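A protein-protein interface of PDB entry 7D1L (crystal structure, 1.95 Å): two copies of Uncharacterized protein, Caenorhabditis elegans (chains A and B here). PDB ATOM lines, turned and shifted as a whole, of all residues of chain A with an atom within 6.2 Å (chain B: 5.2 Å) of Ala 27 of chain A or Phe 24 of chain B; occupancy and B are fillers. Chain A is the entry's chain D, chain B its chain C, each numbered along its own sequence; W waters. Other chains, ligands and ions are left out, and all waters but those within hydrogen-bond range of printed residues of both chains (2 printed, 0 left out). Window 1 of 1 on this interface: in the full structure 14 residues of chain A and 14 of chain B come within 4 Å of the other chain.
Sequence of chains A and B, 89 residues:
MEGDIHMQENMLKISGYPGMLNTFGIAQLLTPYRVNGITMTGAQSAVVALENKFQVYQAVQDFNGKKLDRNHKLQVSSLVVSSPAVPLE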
ATOM      1  N   ASN A  22      -3.042   6.813  19.029  1.00  0.00           N
ATOM      2  CA  ASN A  22      -1.891   7.319  19.756  1.00  0.00           C
ATOM      3  C   ASN A  22      -2.372   7.940  21.068  1.00  0.00           C
ATOM      4  O   ASN A  22      -3.557   7.890  21.417  1.00  0.00           O
ATOM      5  CB  ASN A  22      -1.073   8.303  18.901  1.00  0.00           C
ATOM      6  CG  ASN A  22      -1.853   9.562  18.507  1.00  0.00           C
ATOM      7  OD1 ASN A  22      -2.845   9.926  19.132  1.00  0.00           O
ATOM      8  ND2 ASN A  22      -1.384  10.233  17.459  1.00  0.00           N
ATOM      9  N   THR A  23      -1.431   8.514  21.818  1.00  0.00           N
ATOM     10  CA  THR A  23      -1.774   9.059  23.124  1.00  0.00           C
ATOM     11  C   THR A  23      -2.803  10.180  23.002  1.00  0.00           C
ATOM     12  O   THR A  23      -3.696  10.305  23.847  1.00  0.00           O
ATOM     13  CB  THR A  23      -0.510   9.555  23.838  1.00  0.00           C
ATOM     14  OG1 THR A  23      -0.864  10.040  25.128  1.00  0.00           O
ATOM     15  CG2 THR A  23       0.099  10.684  23.101  1.00  0.00           C
ATOM     16  N   PHE A  24      -2.699  11.007  21.961  1.00  0.00           N
ATOM     17  CA  PHE A  24      -3.695  12.059  21.793  1.00  0.00           C
ATOM     18  C   PHE A  24      -5.066  11.459  21.515  1.00  0.00           C
ATOM     19  O   PHE A  24      -6.078  11.969  22.003  1.00  0.00           O
ATOM     20  CB  PHE A  24      -3.286  13.010  20.673  1.00  0.00           C
ATOM     21  CG  PHE A  24      -2.142  13.918  21.031  1.00  0.00           C
ATOM     22  CD1 PHE A  24      -2.231  14.778  22.115  1.00  0.00           C
ATOM     23  CD2 PHE A  24      -0.988  13.921  20.275  1.00  0.00           C
ATOM     24  CE1 PHE A  24      -1.183  15.627  22.433  1.00  0.00           C
ATOM     25  CE2 PHE A  24       0.066  14.773  20.590  1.00  0.00           C
ATOM     26  CZ  PHE A  24      -0.034  15.623  21.666  1.00  0.00           C
ATOM     27  N   GLY A  25      -5.116  10.372  20.742  1.00  0.00           N
ATOM     28  CA  GLY A  25      -6.394   9.717  20.490  1.00  0.00           C
ATOM     29  C   GLY A  25      -7.016   9.134  21.752  1.00  0.00           C
ATOM     30  O   GLY A  25      -8.238   9.156  21.921  1.00  0.00           O
ATOM     31  N   ILE A  26      -6.188   8.608  22.658  1.00  0.00           N
ATOM     32  CA  ILE A  26      -6.723   8.114  23.922  1.00  0.00           C
ATOM     33  C   ILE A  26      -7.293   9.268  24.748  1.00  0.00           C
ATOM     34  O   ILE A  26      -8.365   9.145  25.359  1.00  0.00           O
ATOM     35  CB  ILE A  26      -5.644   7.323  24.691  1.00  0.00           C
ATOM     36  CG1 ILE A  26      -5.224   6.084  23.896  1.00  0.00           C
ATOM     37  CG2 ILE A  26      -6.153   6.913  26.076  1.00  0.00           C
ATOM     38  CD1 ILE A  26      -3.834   5.523  24.281  1.00  0.00           C
ATOM     39  N   ALA A  27      -6.605  10.412  24.760  1.00  0.00           N
ATOM     40  CA  ALA A  27      -7.134  11.585  25.456  1.00  0.00           C
ATOM     41  C   ALA A  27      -8.477  12.013  24.874  1.00  0.00           C
ATOM     42  O   ALA A  27      -9.388  12.415  25.615  1.00  0.00           O
ATOM     43  CB  ALA A  27      -6.128  12.736  25.384  1.00  0.00           C
ATOM     44  N   GLN A  28      -8.620  11.933  23.545  1.00  0.00           N
ATOM     45  CA  GLN A  28      -9.885  12.313  22.929  1.00  0.00           C
ATOM     46  C   GLN A  28     -11.011  11.379  23.348  1.00  0.00           C
ATOM     47  O   GLN A  28     -12.162  11.815  23.440  1.00  0.00           O
ATOM     48  CB  GLN A  28      -9.750  12.335  21.408  1.00  0.00           C
ATOM     49  CG  GLN A  28      -8.974  13.542  20.887  1.00  0.00           C
ATOM     50  CD  GLN A  28      -8.538  13.366  19.437  1.00  0.00           C
ATOM     51  OE1 GLN A  28      -8.135  12.267  19.028  1.00  0.00           O
ATOM     52  NE2 GLN A  28      -8.585  14.443  18.664  1.00  0.00           N
ATOM     53  N   LEU A  29     -10.698  10.100  23.621  1.00  0.00           N
ATOM     54  CA  LEU A  29     -11.710   9.175  24.137  1.00  0.00           C
ATOM     55  C   LEU A  29     -12.293   9.652  25.457  1.00  0.00           C
ATOM     56  O   LEU A  29     -13.456   9.368  25.758  1.00  0.00           O
ATOM     57  CB  LEU A  29     -11.120   7.782  24.364  1.00  0.00           C
ATOM     58  CG  LEU A  29     -10.753   6.898  23.188  1.00  0.00           C
ATOM     59  CD1 LEU A  29     -10.140   5.626  23.744  1.00  0.00           C
ATOM     60  CD2 LEU A  29     -11.982   6.608  22.358  1.00  0.00           C
ATOM     61  N   LEU A  30     -11.493  10.337  26.270  1.00  0.00           N
ATOM     62  CA  LEU A  30     -11.870  10.722  27.623  1.00  0.00           C
ATOM     63  C   LEU A  30     -12.464  12.125  27.706  1.00  0.00           C
ATOM     64  O   LEU A  30     -12.665  12.630  28.813  1.00  0.00           O
ATOM     65  CB  LEU A  30     -10.652  10.619  28.541  1.00  0.00           C
ATOM     66  CG  LEU A  30     -10.090   9.204  28.605  1.00  0.00           C
ATOM     67  CD1 LEU A  30      -8.697   9.210  29.196  1.00  0.00           C
ATOM     68  CD2 LEU A  30     -11.015   8.336  29.439  1.00  0.00           C
ATOM     69  N   THR A  31     -12.709  12.773  26.577  1.00  0.00           N
ATOM     70  CA  THR A  31     -13.371  14.066  26.596  1.00  0.00           C
ATOM     71  C   THR A  31     -14.665  13.965  27.408  1.00  0.00           C
ATOM     72  O   THR A  31     -15.404  12.981  27.267  1.00  0.00           O
ATOM     73  CB  THR A  31     -13.668  14.506  25.157  1.00  0.00           C
ATOM     74  OG1 THR A  31     -12.451  14.465  24.406  1.00  0.00           O
ATOM     75  CG2 THR A  31     -14.232  15.927  25.104  1.00  0.00           C
ATOM     76  N   TYR A  33     -12.954  15.085  30.250  1.00  0.00           N
ATOM     77  CA  TYR A  33     -12.169  15.075  31.477  1.00  0.00           C
ATOM     78  C   TYR A  33     -10.736  15.548  31.234  1.00  0.00           C
ATOM     79  O   TYR A  33     -10.166  15.378  30.154  1.00  0.00           O
ATOM     80  CB  TYR A  33     -12.198  13.676  32.105  1.00  0.00           C
ATOM     81  CG  TYR A  33     -13.615  13.334  32.464  1.00  0.00           C
ATOM     82  CD1 TYR A  33     -14.238  13.965  33.530  1.00  0.00           C
ATOM     83  CD2 TYR A  33     -14.367  12.460  31.683  1.00  0.00           C
ATOM     84  CE1 TYR A  33     -15.556  13.698  33.854  1.00  0.00           C
ATOM     85  CE2 TYR A  33     -15.691  12.181  31.998  1.00  0.00           C
ATOM     86  CZ  TYR A  33     -16.279  12.805  33.085  1.00  0.00           C
ATOM     87  OH  TYR A  33     -17.601  12.566  33.413  1.00  0.00           O
ATOM     88  N   VAL A  35      -7.045  15.306  31.183  1.00  0.00           N
ATOM     89  CA  VAL A  35      -6.025  14.272  31.125  1.00  0.00           C
ATOM     90  C   VAL A  35      -4.671  14.933  31.310  1.00  0.00           C
ATOM     91  O   VAL A  35      -4.325  15.856  30.569  1.00  0.00           O
ATOM     92  CB  VAL A  35      -6.093  13.521  29.788  1.00  0.00           C
ATOM     93  CG1 VAL A  35      -4.945  12.505  29.670  1.00  0.00           C
ATOM     94  CG2 VAL A  35      -7.459  12.856  29.635  1.00  0.00           C
ATOM     95  N   ASN A  36      -3.898  14.457  32.288  1.00  0.00           N
ATOM     96  CA  ASN A  36      -2.588  15.020  32.580  1.00  0.00           C
ATOM     97  C   ASN A  36      -1.436  14.113  32.178  1.00  0.00           C
ATOM     98  O   ASN A  36      -0.294  14.579  32.119  1.00  0.00           O
ATOM     99  CB  ASN A  36      -2.462  15.356  34.074  1.00  0.00           C
ATOM    100  CG  ASN A  36      -3.275  16.568  34.459  1.00  0.00           C
ATOM    101  OD1 ASN A  36      -3.523  17.446  33.632  1.00  0.00           O
ATOM    102  ND2 ASN A  36      -3.727  16.611  35.708  1.00  0.00           N
ATOM    103  N   GLY A  37      -1.700  12.850  31.879  1.00  0.00           N
ATOM    104  CA  GLY A  37      -0.650  11.949  31.457  1.00  0.00           C
ATOM    105  C   GLY A  37      -1.215  10.629  30.972  1.00  0.00           C
ATOM    106  O   GLY A  37      -2.251  10.177  31.464  1.00  0.00           O
ATOM    107  N   ILE A  38      -0.565  10.019  29.987  1.00  0.00           N
ATOM    108  CA  ILE A  38      -0.989   8.742  29.427  1.00  0.00           C
ATOM    109  C   ILE A  38       0.263   7.927  29.186  1.00  0.00           C
ATOM    110  O   ILE A  38       1.221   8.422  28.585  1.00  0.00           O
ATOM    111  CB  ILE A  38      -1.780   8.894  28.105  1.00  0.00           C
ATOM    112  CG1 ILE A  38      -3.054   9.737  28.305  1.00  0.00           C
ATOM    113  CG2 ILE A  38      -2.135   7.513  27.534  1.00  0.00           C
ATOM    114  CD1 ILE A  38      -3.918   9.876  27.048  1.00  0.00           C
ATOM    115  N   ASN B  22      -4.143  21.949  28.684  1.00  0.00           N
ATOM    116  CA  ASN B  22      -2.839  21.407  28.316  1.00  0.00           C
ATOM    117  C   ASN B  22      -2.940  20.816  26.903  1.00  0.00           C
ATOM    118  O   ASN B  22      -3.965  20.969  26.221  1.00  0.00           O
ATOM    119  CB  ASN B  22      -2.359  20.398  29.373  1.00  0.00           C
ATOM    120  CG  ASN B  22      -3.331  19.242  29.582  1.00  0.00           C
ATOM    121  OD1 ASN B  22      -4.225  18.994  28.760  1.00  0.00           O
ATOM    122  ND2 ASN B  22      -3.151  18.517  30.680  1.00  0.00           N
ATOM    123  N   THR B  23      -1.870  20.157  26.433  1.00  0.00           N
ATOM    124  CA  THR B  23      -1.889  19.641  25.064  1.00  0.00           C
ATOM    125  C   THR B  23      -2.944  18.556  24.904  1.00  0.00           C
ATOM    126  O   THR B  23      -3.555  18.438  23.841  1.00  0.00           O
ATOM    127  CB  THR B  23      -0.524  19.086  24.640  1.00  0.00           C
ATOM    128  OG1 THR B  23      -0.128  18.049  25.544  1.00  0.00           O
ATOM    129  CG2 THR B  23       0.540  20.184  24.611  1.00  0.00           C
ATOM    130  N   PHE B  24      -3.165  17.737  25.938  1.00  0.00           N
ATOM    131  CA  PHE B  24      -4.247  16.759  25.840  1.00  0.00           C
ATOM    132  C   PHE B  24      -5.600  17.453  25.685  1.00  0.00           C
ATOM    133  O   PHE B  24      -6.465  16.989  24.931  1.00  0.00           O
ATOM    134  CB  PHE B  24      -4.245  15.840  27.060  1.00  0.00           C
ATOM    135  CG  PHE B  24      -3.082  14.882  27.103  1.00  0.00           C
ATOM    136  CD1 PHE B  24      -2.857  13.998  26.070  1.00  0.00           C
ATOM    137  CD2 PHE B  24      -2.209  14.884  28.184  1.00  0.00           C
ATOM    138  CE1 PHE B  24      -1.795  13.101  26.115  1.00  0.00           C
ATOM    139  CE2 PHE B  24      -1.140  13.997  28.234  1.00  0.00           C
ATOM    140  CZ  PHE B  24      -0.934  13.106  27.193  1.00  0.00           C
ATOM    141  N   GLY B  25      -5.793  18.578  26.377  1.00  0.00           N
ATOM    142  CA  GLY B  25      -7.047  19.310  26.246  1.00  0.00           C
ATOM    143  C   GLY B  25      -7.227  19.908  24.862  1.00  0.00           C
ATOM    144  O   GLY B  25      -8.339  19.950  24.330  1.00  0.00           O
ATOM    145  N   ILE B  26      -6.139  20.364  24.250  1.00  0.00           N
ATOM    146  CA  ILE B  26      -6.241  20.868  22.888  1.00  0.00           C
ATOM    147  C   ILE B  26      -6.600  19.741  21.924  1.00  0.00           C
ATOM    148  O   ILE B  26      -7.434  19.922  21.028  1.00  0.00           O
ATOM    149  CB  ILE B  26      -4.939  21.584  22.493  1.00  0.00           C
ATOM    150  CG1 ILE B  26      -4.735  22.810  23.404  1.00  0.00           C
ATOM    151  CG2 ILE B  26      -4.977  21.990  21.017  1.00  0.00           C
ATOM    152  CD1 ILE B  26      -3.292  23.278  23.476  1.00  0.00           C
ATOM    153  N   ALA B  27      -6.004  18.556  22.104  1.00  0.00           N
ATOM    154  CA  ALA B  27      -6.371  17.420  21.255  1.00  0.00           C
ATOM    155  C   ALA B  27      -7.847  17.074  21.402  1.00  0.00           C
ATOM    156  O   ALA B  27      -8.512  16.728  20.419  1.00  0.00           O
ATOM    157  CB  ALA B  27      -5.502  16.195  21.579  1.00  0.00           C
ATOM    158  N   GLN B  28      -8.377  17.150  22.631  1.00  0.00           N
ATOM    159  CA  GLN B  28      -9.796  16.872  22.840  1.00  0.00           C
ATOM    160  C   GLN B  28     -10.681  17.856  22.089  1.00  0.00           C
ATOM    161  O   GLN B  28     -11.759  17.476  21.620  1.00  0.00           O
ATOM    162  CB  GLN B  28     -10.130  16.892  24.331  1.00  0.00           C
ATOM    163  CG  GLN B  28      -9.516  15.731  25.110  1.00  0.00           C
ATOM    164  CD  GLN B  28      -9.732  15.881  26.611  1.00  0.00           C
ATOM    165  OE1 GLN B  28      -9.784  17.003  27.123  1.00  0.00           O
ATOM    166  NE2 GLN B  28      -9.880  14.757  27.320  1.00  0.00           N
HETATM  167  O   HOH W   1      -1.028  19.134  32.643  1.00  0.00           O
HETATM  168  O   HOH W   2      -6.957  17.320  29.099  1.00  0.00           O
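The side-chain amide nitrogen of Asn 22 of chain B is in hydrogen-bond range of the backbone carbonyl oxygen of Val 35 of chain A. The side-chain amide nitrogen of Asn 22 of chain B sits at hydrogen-bond distance from the side-chain amide oxygen of Asn 36 of chain A (3.2 Å). The side-chain amide nitrogen (NE2) of Gln 28 of chain A sits at hydrogen-bond distance from the backbone carbonyl oxygen (O) of Ala 27 of chain B, 2.9 Å away. The backbone carbonyl oxygen (O) of Ala 27 of chain A lies within hydrogen-bond range of the side-chain amide nitrogen (NE2) of Gln 28 of chain B. The side-chain amide nitrogen of Gln 28 of chain B sits at hydrogen-bond distance from the backbone carbonyl oxygen of Tyr 33 of chain A (2.9 Å).
OD1 of Asn 22 of chain B sits close to N of Phe 24 of chain B, 3.3 Å away. OD1 of Asn 22 of chain B is in hydrogen-bond range of N of Gly 25 of chain B. OD1 of Asn 22 of chain A lies within hydrogen-bond range of N of Phe 24 of chain A, 3.0 Å away. The side-chain hydroxyl (OG1) of Thr 31 of chain A is in hydrogen-bond range of the backbone carbonyl oxygen (O) of Gln 28 of chain A (2.8 Å).
Phe 24 of chain B touches Thr 23 of chain A. CE1 of Phe 24 of chain A touches O of Thr 23 of chain B, at 3.9 Å. Ala 27 of chain B touches Phe 24 of chain A (CB to CD1, 3.6 Å). Gln 28 of chain A touches Gln 28 of chain B. Gln 28 of chain B touches Leu 30 of chain A. OG1 of Thr 31 of chain A touches CG of Gln 28 of chain B, 3.3 Å away. Val 35 of chain A touches Phe 24 of chain B (O to CD2, 3.3 Å). Gln 28 of chain B touches Val 35 of chain A (NE2 to CG2, 3.9 Å). Asn 36 of chain A touches Phe 24 of chain B. Phe 24 of chain B touches Gly 37 of chain A.
Of the printed residues of chain B, Phe 24 of chain A touches Thr 23 and Ala 27. Ile 26 of chain A touches none of the printed residues of chain B. Of chain B, only Phe 24 and Gln 28 come within 4 Å of Ala 27 of chain A. Of the printed residues of chain B, Thr 31 of chain A touches Gln 28. Of the printed residues of chain B, Asn 36 of chain A touches Asn 22 and Phe 24. Of the printed residues of chain A, Thr 23 of chain B touches Phe 24 (3.9 Å). Phe 24 of chain B touches just these residues of chain A: Thr 23 (3.3 Å), Ala 27 (3.6 Å), Val 35 (3.3 Å), Asn 36 (3.96 Å), Gly 37 (3.8 Å) and Ile 38 (3.97 Å).
Of the 7 printed residues of chain B, 5 touch a printed residue of chain A. Hydrophobic or aromatic side chains of chain B that line the printed part of chain A: Phe 24 and Ala 27. Of the 15 printed residues of chain A, 11 touch a printed residue of chain B. Printed residues of chain A that touch a printed residue of chain B: Thr 23, Phe 24, Ala 27, Gln 28, Leu 30, Thr 31, Tyr 33, Val 35, Asn 36, Gly 37 and Ile 38. Along chain A the printed residues that touch a printed residue of chain B span positions 23 to 38. Among the printed residues, 17 pairs touch across the chains. Among the printed residues, no Asp or Glu carboxylate lies within 4 Å of a Lys or Arg side-chain nitrogen of the other chain.
Thr 23 of chain A touches Phe 24 of chain B, and with the chains exchanged Phe 24 of chain A touches Thr 23 of chain B. Phe 24 of chain A touches Ala 27 of chain B, and with the chains exchanged Ala 27 of chain A touches Phe 24 of chain B. Ala 27 of chain A touches Gln 28 of chain B, and with the chains exchanged Gln 28 of chain A touches Ala 27 of chain B. Gln 28 of chain B touches its own counterpart, Gln 28 of chain A. 7 positions are printed for both chains. Of the 17 pairs that touch across the chains among the printed residues, 7 have their exchanged pair printed and touching as well.
Water W2 lies within hydrogen-bond range of the backbone NH (N) of Val 35 of chain A (2.9 Å), the backbone NH (N) of Gly 25 of chain B (3.2 Å), the side-chain amide oxygen (OD1) of Asn 22 of chain B (3.2 Å) and the side-chain amide oxygen (OE1) of Gln 28 of chain B (3.5 Å). Water W1 lies within hydrogen-bond range of ND2 of Asn 22 of chain B and OD1 of Asn 36 of chain A.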
